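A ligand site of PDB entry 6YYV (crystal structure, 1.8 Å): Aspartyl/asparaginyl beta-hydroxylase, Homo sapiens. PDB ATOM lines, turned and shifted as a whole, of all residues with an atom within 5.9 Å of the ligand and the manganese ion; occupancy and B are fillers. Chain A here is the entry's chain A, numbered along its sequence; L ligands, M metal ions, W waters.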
ATOM      1  N   LEU A 290     -29.427   2.874  33.123  1.00  0.00           N
ATOM      2  CA  LEU A 290     -28.119   2.690  32.481  1.00  0.00           C
ATOM      3  C   LEU A 290     -27.723   3.851  31.584  1.00  0.00           C
ATOM      4  O   LEU A 290     -26.539   3.975  31.206  1.00  0.00           O
ATOM      5  CB  LEU A 290     -28.148   1.413  31.649  1.00  0.00           C
ATOM      6  CG  LEU A 290     -28.348   0.166  32.503  1.00  0.00           C
ATOM      7  CD1 LEU A 290     -28.277  -1.110  31.694  1.00  0.00           C
ATOM      8  CD2 LEU A 290     -27.291   0.083  33.632  1.00  0.00           C
ATOM      9  N   TRP A 296     -31.118   6.374  23.080  1.00  0.00           N
ATOM     10  CA  TRP A 296     -30.734   4.967  22.975  1.00  0.00           C
ATOM     11  C   TRP A 296     -32.010   4.151  23.060  1.00  0.00           C
ATOM     12  O   TRP A 296     -32.769   4.296  24.024  1.00  0.00           O
ATOM     13  CB  TRP A 296     -29.749   4.617  24.107  1.00  0.00           C
ATOM     14  CG  TRP A 296     -29.328   3.171  24.341  1.00  0.00           C
ATOM     15  CD1 TRP A 296     -29.086   2.206  23.407  1.00  0.00           C
ATOM     16  CD2 TRP A 296     -29.103   2.565  25.621  1.00  0.00           C
ATOM     17  NE1 TRP A 296     -28.757   1.027  24.024  1.00  0.00           N
ATOM     18  CE2 TRP A 296     -28.749   1.219  25.384  1.00  0.00           C
ATOM     19  CE3 TRP A 296     -29.188   3.010  26.960  1.00  0.00           C
ATOM     20  CZ2 TRP A 296     -28.500   0.326  26.425  1.00  0.00           C
ATOM     21  CZ3 TRP A 296     -28.919   2.111  27.980  1.00  0.00           C
ATOM     22  CH2 TRP A 296     -28.578   0.798  27.710  1.00  0.00           C
ATOM     23  N   SER A 339     -30.585  -2.327  18.209  1.00  0.00           N
ATOM     24  CA  SER A 339     -30.178  -1.382  19.244  1.00  0.00           C
ATOM     25  C   SER A 339     -29.590  -0.154  18.571  1.00  0.00           C
ATOM     26  O   SER A 339     -28.576  -0.263  17.871  1.00  0.00           O
ATOM     27  CB  SER A 339     -29.178  -2.019  20.183  1.00  0.00           C
ATOM     28  OG  SER A 339     -28.985  -1.196  21.328  1.00  0.00           O
ATOM     29  N   ILE A 340     -30.232   0.979  18.708  1.00  0.00           N
ATOM     30  CA  ILE A 340     -29.798   2.228  18.103  1.00  0.00           C
ATOM     31  C   ILE A 340     -29.338   3.204  19.186  1.00  0.00           C
ATOM     32  O   ILE A 340     -29.950   3.317  20.253  1.00  0.00           O
ATOM     33  CB  ILE A 340     -30.905   2.837  17.220  1.00  0.00           C
ATOM     34  CG1 ILE A 340     -30.368   4.052  16.438  1.00  0.00           C
ATOM     35  CG2 ILE A 340     -32.099   3.289  18.017  1.00  0.00           C
ATOM     36  CD1 ILE A 340     -31.249   4.479  15.265  1.00  0.00           C
ATOM     37  N   MET A 341     -28.293   3.956  18.866  1.00  0.00           N
ATOM     38  CA  MET A 341     -27.673   4.870  19.824  1.00  0.00           C
ATOM     39  C   MET A 341     -27.205   6.093  19.047  1.00  0.00           C
ATOM     40  O   MET A 341     -26.593   5.966  17.984  1.00  0.00           O
ATOM     41  CB  MET A 341     -26.528   4.187  20.594  1.00  0.00           C
ATOM     42  CG  MET A 341     -26.067   4.958  21.849  1.00  0.00           C
ATOM     43  SD  MET A 341     -24.701   4.176  22.698  1.00  0.00           S
ATOM     44  CE  MET A 341     -25.495   2.677  23.231  1.00  0.00           C
ATOM     45  N   VAL A 347     -23.595   5.003  28.199  1.00  0.00           N
ATOM     46  CA  VAL A 347     -24.210   3.959  29.003  1.00  0.00           C
ATOM     47  C   VAL A 347     -23.248   3.664  30.147  1.00  0.00           C
ATOM     48  O   VAL A 347     -22.082   3.298  29.928  1.00  0.00           O
ATOM     49  CB  VAL A 347     -24.489   2.706  28.160  1.00  0.00           C
ATOM     50  CG1 VAL A 347     -25.101   1.614  28.998  1.00  0.00           C
ATOM     51  CG2 VAL A 347     -25.386   3.054  26.949  1.00  0.00           C
ATOM     52  N   HIS A 350     -21.957  -1.586  33.577  1.00  0.00           N
ATOM     53  CA  HIS A 350     -22.902  -2.504  34.185  1.00  0.00           C
ATOM     54  C   HIS A 350     -22.586  -3.897  33.717  1.00  0.00           C
ATOM     55  O   HIS A 350     -21.789  -4.103  32.816  1.00  0.00           O
ATOM     56  CB  HIS A 350     -24.361  -2.190  33.794  1.00  0.00           C
ATOM     57  CG  HIS A 350     -24.631  -2.335  32.337  1.00  0.00           C
ATOM     58  ND1 HIS A 350     -24.253  -1.366  31.420  1.00  0.00           N
ATOM     59  CD2 HIS A 350     -25.190  -3.339  31.599  1.00  0.00           C
ATOM     60  CE1 HIS A 350     -24.573  -1.770  30.194  1.00  0.00           C
ATOM     61  NE2 HIS A 350     -25.145  -2.954  30.274  1.00  0.00           N
ATOM     62  N   THR A 351     -23.262  -4.863  34.329  1.00  0.00           N
ATOM     63  CA  THR A 351     -23.288  -6.218  33.826  1.00  0.00           C
ATOM     64  C   THR A 351     -24.721  -6.679  33.592  1.00  0.00           C
ATOM     65  O   THR A 351     -25.664  -6.112  34.145  1.00  0.00           O
ATOM     66  CB  THR A 351     -22.622  -7.253  34.761  1.00  0.00           C
ATOM     67  OG1 THR A 351     -23.514  -7.708  35.806  1.00  0.00           O
ATOM     68  CG2 THR A 351     -21.349  -6.719  35.450  1.00  0.00           C
ATOM     69  N   GLY A 352     -24.856  -7.735  32.778  1.00  0.00           N
ATOM     70  CA  GLY A 352     -26.093  -8.446  32.660  1.00  0.00           C
ATOM     71  C   GLY A 352     -26.384  -9.356  33.843  1.00  0.00           C
ATOM     72  O   GLY A 352     -25.641  -9.464  34.815  1.00  0.00           O
ATOM     73  N   ARG A 357     -25.226 -16.802  29.179  1.00  0.00           N
ATOM     74  CA  ARG A 357     -25.381 -16.378  27.795  1.00  0.00           C
ATOM     75  C   ARG A 357     -24.131 -15.682  27.321  1.00  0.00           C
ATOM     76  O   ARG A 357     -23.357 -15.138  28.098  1.00  0.00           O
ATOM     77  CB  ARG A 357     -26.533 -15.399  27.612  1.00  0.00           C
ATOM     78  CG  ARG A 357     -26.258 -14.030  28.195  1.00  0.00           C
ATOM     79  CD  ARG A 357     -27.512 -13.220  28.156  1.00  0.00           C
ATOM     80  NE  ARG A 357     -27.334 -11.803  28.458  1.00  0.00           N
ATOM     81  CZ  ARG A 357     -28.317 -10.987  28.863  1.00  0.00           C
ATOM     82  NH1 ARG A 357     -29.532 -11.460  28.996  1.00  0.00           N
ATOM     83  NH2 ARG A 357     -28.119  -9.686  29.082  1.00  0.00           N
ATOM     84  N   ARG A 359     -23.196 -12.611  24.335  1.00  0.00           N
ATOM     85  CA  ARG A 359     -23.858 -11.543  23.613  1.00  0.00           C
ATOM     86  C   ARG A 359     -23.072 -11.208  22.343  1.00  0.00           C
ATOM     87  O   ARG A 359     -21.926 -10.727  22.395  1.00  0.00           O
ATOM     88  CB  ARG A 359     -24.042 -10.317  24.498  1.00  0.00           C
ATOM     89  CG  ARG A 359     -24.664  -9.104  23.788  1.00  0.00           C
ATOM     90  CD  ARG A 359     -25.414  -8.293  24.834  1.00  0.00           C
ATOM     91  NE  ARG A 359     -26.699  -8.870  25.195  1.00  0.00           N
ATOM     92  CZ  ARG A 359     -27.671  -8.200  25.857  1.00  0.00           C
ATOM     93  NH1 ARG A 359     -27.510  -6.950  26.310  1.00  0.00           N
ATOM     94  NH2 ARG A 359     -28.823  -8.789  26.065  1.00  0.00           N
ATOM     95  N   HIS A 361     -22.932  -8.907  18.864  1.00  0.00           N
ATOM     96  CA  HIS A 361     -23.300  -7.643  18.258  1.00  0.00           C
ATOM     97  C   HIS A 361     -22.922  -7.702  16.793  1.00  0.00           C
ATOM     98  O   HIS A 361     -21.737  -7.888  16.468  1.00  0.00           O
ATOM     99  CB  HIS A 361     -22.535  -6.490  18.897  1.00  0.00           C
ATOM    100  CG  HIS A 361     -23.078  -6.019  20.192  1.00  0.00           C
ATOM    101  ND1 HIS A 361     -22.548  -4.924  20.862  1.00  0.00           N
ATOM    102  CD2 HIS A 361     -24.059  -6.509  20.995  1.00  0.00           C
ATOM    103  CE1 HIS A 361     -23.186  -4.773  22.003  1.00  0.00           C
ATOM    104  NE2 HIS A 361     -24.108  -5.716  22.101  1.00  0.00           N
ATOM    105  N   ILE A 373     -17.046   0.242  22.638  1.00  0.00           N
ATOM    106  CA  ILE A 373     -17.557  -0.607  23.697  1.00  0.00           C
ATOM    107  C   ILE A 373     -16.380  -1.223  24.443  1.00  0.00           C
ATOM    108  O   ILE A 373     -15.519  -1.870  23.829  1.00  0.00           O
ATOM    109  CB  ILE A 373     -18.504  -1.693  23.153  1.00  0.00           C
ATOM    110  CG1 ILE A 373     -18.853  -2.643  24.305  1.00  0.00           C
ATOM    111  CG2 ILE A 373     -17.905  -2.425  21.945  1.00  0.00           C
ATOM    112  CD1 ILE A 373     -20.017  -3.531  23.920  1.00  0.00           C
ATOM    113  N   TRP A 382     -17.153  -1.428  16.650  1.00  0.00           N
ATOM    114  CA  TRP A 382     -17.933  -2.236  15.745  1.00  0.00           C
ATOM    115  C   TRP A 382     -17.470  -1.994  14.313  1.00  0.00           C
ATOM    116  O   TRP A 382     -16.890  -0.958  14.008  1.00  0.00           O
ATOM    117  CB  TRP A 382     -19.420  -1.866  15.893  1.00  0.00           C
ATOM    118  CG  TRP A 382     -20.023  -2.148  17.231  1.00  0.00           C
ATOM    119  CD1 TRP A 382     -20.564  -3.352  17.658  1.00  0.00           C
ATOM    120  CD2 TRP A 382     -20.172  -1.220  18.319  1.00  0.00           C
ATOM    121  NE1 TRP A 382     -21.045  -3.216  18.951  1.00  0.00           N
ATOM    122  CE2 TRP A 382     -20.801  -1.936  19.377  1.00  0.00           C
ATOM    123  CE3 TRP A 382     -19.818   0.120  18.517  1.00  0.00           C
ATOM    124  CZ2 TRP A 382     -21.064  -1.360  20.598  1.00  0.00           C
ATOM    125  CZ3 TRP A 382     -20.111   0.701  19.755  1.00  0.00           C
ATOM    126  CH2 TRP A 382     -20.750  -0.031  20.765  1.00  0.00           C
ATOM    127  N   PHE A 390     -19.079 -10.790  23.173  1.00  0.00           N
ATOM    128  CA  PHE A 390     -18.591 -10.573  24.531  1.00  0.00           C
ATOM    129  C   PHE A 390     -19.504 -11.252  25.549  1.00  0.00           C
ATOM    130  O   PHE A 390     -20.661 -11.599  25.270  1.00  0.00           O
ATOM    131  CB  PHE A 390     -18.394  -9.071  24.863  1.00  0.00           C
ATOM    132  CG  PHE A 390     -19.664  -8.274  24.968  1.00  0.00           C
ATOM    133  CD1 PHE A 390     -20.275  -7.827  23.826  1.00  0.00           C
ATOM    134  CD2 PHE A 390     -20.150  -7.887  26.186  1.00  0.00           C
ATOM    135  CE1 PHE A 390     -21.455  -7.045  23.880  1.00  0.00           C
ATOM    136  CE2 PHE A 390     -21.292  -7.100  26.280  1.00  0.00           C
ATOM    137  CZ  PHE A 390     -21.973  -6.712  25.141  1.00  0.00           C
ATOM    138  N   ASP A 392     -21.459 -10.656  28.580  1.00  0.00           N
ATOM    139  CA  ASP A 392     -21.959  -9.444  29.207  1.00  0.00           C
ATOM    140  C   ASP A 392     -22.224  -9.594  30.711  1.00  0.00           C
ATOM    141  O   ASP A 392     -22.647  -8.623  31.370  1.00  0.00           O
ATOM    142  CB  ASP A 392     -23.203  -8.937  28.423  1.00  0.00           C
ATOM    143  CG  ASP A 392     -24.523  -9.517  28.892  1.00  0.00           C
ATOM    144  OD1 ASP A 392     -24.688 -10.741  29.112  1.00  0.00           O
ATOM    145  OD2 ASP A 392     -25.493  -8.719  28.991  1.00  0.00           O
ATOM    146  N   HIS A 396     -19.284  -3.918  31.291  1.00  0.00           N
ATOM    147  CA  HIS A 396     -19.136  -3.297  29.979  1.00  0.00           C
ATOM    148  C   HIS A 396     -19.793  -1.915  30.013  1.00  0.00           C
ATOM    149  O   HIS A 396     -20.596  -1.584  30.887  1.00  0.00           O
ATOM    150  CB  HIS A 396     -19.696  -4.259  28.894  1.00  0.00           C
ATOM    151  CG  HIS A 396     -21.127  -4.653  29.070  1.00  0.00           C
ATOM    152  ND1 HIS A 396     -21.552  -5.670  29.907  1.00  0.00           N
ATOM    153  CD2 HIS A 396     -22.250  -4.166  28.473  1.00  0.00           C
ATOM    154  CE1 HIS A 396     -22.873  -5.732  29.865  1.00  0.00           C
ATOM    155  NE2 HIS A 396     -23.315  -4.859  28.976  1.00  0.00           N
ATOM    156  N   GLU A 397     -19.379  -1.064  29.078  1.00  0.00           N
ATOM    157  CA  GLU A 397     -19.653   0.361  29.075  1.00  0.00           C
ATOM    158  C   GLU A 397     -19.556   0.805  27.633  1.00  0.00           C
ATOM    159  O   GLU A 397     -18.714   0.292  26.885  1.00  0.00           O
ATOM    160  CB  GLU A 397     -18.667   1.130  29.944  1.00  0.00           C
ATOM    161  CG  GLU A 397     -18.900   2.607  30.008  1.00  0.00           C
ATOM    162  CD  GLU A 397     -17.983   3.234  31.012  1.00  0.00           C
ATOM    163  OE1 GLU A 397     -17.121   2.523  31.502  1.00  0.00           O
ATOM    164  OE2 GLU A 397     -18.112   4.419  31.318  1.00  0.00           O
ATOM    165  N   VAL A 398     -20.435   1.718  27.241  1.00  0.00           N
ATOM    166  CA  VAL A 398     -20.554   2.106  25.837  1.00  0.00           C
ATOM    167  C   VAL A 398     -20.620   3.630  25.697  1.00  0.00           C
ATOM    168  O   VAL A 398     -21.278   4.323  26.490  1.00  0.00           O
ATOM    169  CB  VAL A 398     -21.784   1.439  25.171  1.00  0.00           C
ATOM    170  CG1 VAL A 398     -22.036   2.071  23.789  1.00  0.00           C
ATOM    171  CG2 VAL A 398     -21.552  -0.108  25.031  1.00  0.00           C
ATOM    172  N   ARG A 406     -25.904   5.219  15.227  1.00  0.00           N
ATOM    173  CA  ARG A 406     -25.238   3.921  15.244  1.00  0.00           C
ATOM    174  C   ARG A 406     -26.235   2.799  15.502  1.00  0.00           C
ATOM    175  O   ARG A 406     -26.837   2.724  16.586  1.00  0.00           O
ATOM    176  CB  ARG A 406     -24.134   3.888  16.297  1.00  0.00           C
ATOM    177  CG  ARG A 406     -23.390   2.568  16.268  1.00  0.00           C
ATOM    178  CD  ARG A 406     -23.346   1.962  17.691  1.00  0.00           C
ATOM    179  NE  ARG A 406     -24.668   1.541  18.188  1.00  0.00           N
ATOM    180  CZ  ARG A 406     -24.890   0.988  19.370  1.00  0.00           C
ATOM    181  NH1 ARG A 406     -23.914   0.735  20.230  1.00  0.00           N
ATOM    182  NH2 ARG A 406     -26.129   0.638  19.697  1.00  0.00           N
ATOM    183  N   ILE A 408     -26.835  -1.367  15.702  1.00  0.00           N
ATOM    184  CA  ILE A 408     -26.299  -2.717  15.813  1.00  0.00           C
ATOM    185  C   ILE A 408     -27.473  -3.681  15.969  1.00  0.00           C
ATOM    186  O   ILE A 408     -28.598  -3.288  16.313  1.00  0.00           O
ATOM    187  CB  ILE A 408     -25.292  -2.842  16.996  1.00  0.00           C
ATOM    188  CG1 ILE A 408     -26.052  -2.744  18.341  1.00  0.00           C
ATOM    189  CG2 ILE A 408     -24.157  -1.835  16.840  1.00  0.00           C
ATOM    190  CD1 ILE A 408     -25.147  -2.914  19.548  1.00  0.00           C
ATOM    191  N   ILE A 410     -28.258  -7.163  18.149  1.00  0.00           N
ATOM    192  CA  ILE A 410     -27.843  -7.880  19.358  1.00  0.00           C
ATOM    193  C   ILE A 410     -28.488  -9.264  19.395  1.00  0.00           C
ATOM    194  O   ILE A 410     -29.725  -9.406  19.337  1.00  0.00           O
ATOM    195  CB  ILE A 410     -28.208  -7.091  20.642  1.00  0.00           C
ATOM    196  CG1 ILE A 410     -27.544  -5.729  20.670  1.00  0.00           C
ATOM    197  CG2 ILE A 410     -27.732  -7.830  21.895  1.00  0.00           C
ATOM    198  CD1 ILE A 410     -27.756  -4.907  21.893  1.00  0.00           C
HETATM  199  C1  LIG L   1     -25.086  -2.928  26.123  1.00  0.00           C
HETATM  200  C2  LIG L   1     -24.863  -1.818  25.006  1.00  0.00           C
HETATM  201  C3  LIG L   1     -25.931  -1.942  23.768  1.00  0.00           C
HETATM  202  C4  LIG L   1     -24.773  -0.400  25.723  1.00  0.00           C
HETATM  203  C5  LIG L   1     -25.217  -4.268  25.761  1.00  0.00           C
HETATM  204  C6  LIG L   1     -25.581  -1.005  22.645  1.00  0.00           C
HETATM  205  O1  LIG L   1     -25.068  -2.679  27.338  1.00  0.00           O
HETATM  206  O2  LIG L   1     -25.421  -5.154  26.627  1.00  0.00           O
HETATM  207  O3  LIG L   1     -25.141  -4.811  24.530  1.00  0.00           O
HETATM  208  O4  LIG L   1     -24.414  -0.719  22.533  1.00  0.00           O
HETATM  209  O5  LIG L   1     -26.634  -0.728  21.879  1.00  0.00           O
HETATM  210 MN    MN M   1     -25.402  -4.382  28.691  1.00  0.00          MN
HETATM  211  O   HOH W   1     -27.519  -3.966  28.471  1.00  0.00           O
HETATM  212  O   HOH W   2     -28.293  -3.959  25.488  1.00  0.00           O
HETATM  213  O   HOH W   3     -26.018  -6.108  29.708  1.00  0.00           O
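An oxygen (O5) of the ligand is in hydrogen-bond range of the side-chain hydroxyl (OG) of Ser 339 (2.5 Å).
The guanidinium group (NH2) of Arg 406 lies within salt-bridge range of an oxygen (O5) of the ligand.
NH1 of Arg 359 is in salt-bridge range of O3 of the ligand (3.7 Å).
An oxygen (O3) of the ligand is in hydrogen-bond range of a ring nitrogen (NE2) of His 361 (2.8 Å).
An oxygen (O5) of the ligand is in hydrogen-bond range of the indole nitrogen (NE1) of Trp 296.
The backbone carbonyl oxygen (O) of Asp 392 lies close to a ring nitrogen (ND1) of His 396 (3.5 Å).
O of Ser 339 is in hydrogen-bond range of NH2 of Arg 406 (3.2 Å).
O of Ile 408 sits at hydrogen-bond distance from N of Ser 339 (2.9 Å).
The backbone carbonyl oxygen (O) of Met 341 sits at hydrogen-bond distance from the backbone NH (N) of Arg 406.
The backbone carbonyl oxygen (O) of Phe 390 lies within hydrogen-bond range of the backbone NH (N) of Arg 359, 2.9 Å away.
The side-chain carboxylate (OD2) of Asp 392 lies within salt-bridge range of the guanidinium group (NH1) of Arg 359 (3.8 Å).
The indole nitrogen (NE1) of Trp 382 is in hydrogen-bond range of a ring nitrogen (ND1) of His 361, at 3.0 Å.
The backbone carbonyl oxygen (O) of Val 398 is in hydrogen-bond range of the backbone NH (N) of Val 347, at 3.0 Å.
Residues that only touch the ligand: Met 341, Val 347, Trp 382, Phe 390, Val 398, Ile 408 and Ile 410.
Hydrophobic or aromatic side chains within 4 Å of the ligand: Trp 296, Met 341, Val 347, His 350, His 361, Trp 382, Phe 390, His 396, Val 398, Ile 408 and Ile 410.
14 residues have an atom within 4 Å of the ligand: Trp 296, Ser 339, Met 341, Val 347, His 350, Arg 359, His 361, Trp 382, Phe 390, His 396, Val 398, Arg 406, Ile 408 and Ile 410.
Along chain A the residues within 4 Å of the ligand span positions 296 to 410.
Within 4 Å of the manganese ion: His 350 and His 396.
The manganese ion is bound by water W3 (2.1 Å).
The manganese ion is bound by a ring nitrogen (NE2) of His 350, at 2.1 Å.
The manganese ion is bound by NE2 of His 396, at 2.2 Å.
The manganese ion is bound by water W1 (2.2 Å).
O1 of the ligand binds the manganese ion, 2.2 Å away.
The manganese ion is bound by O2 of the ligand (2.2 Å).
The manganese ion has six donor atoms within binding distance.
Water W2 bridges the guanidinium group of Arg 359 (3.2 Å) and an oxygen (O3) of the ligand (3.4 Å).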
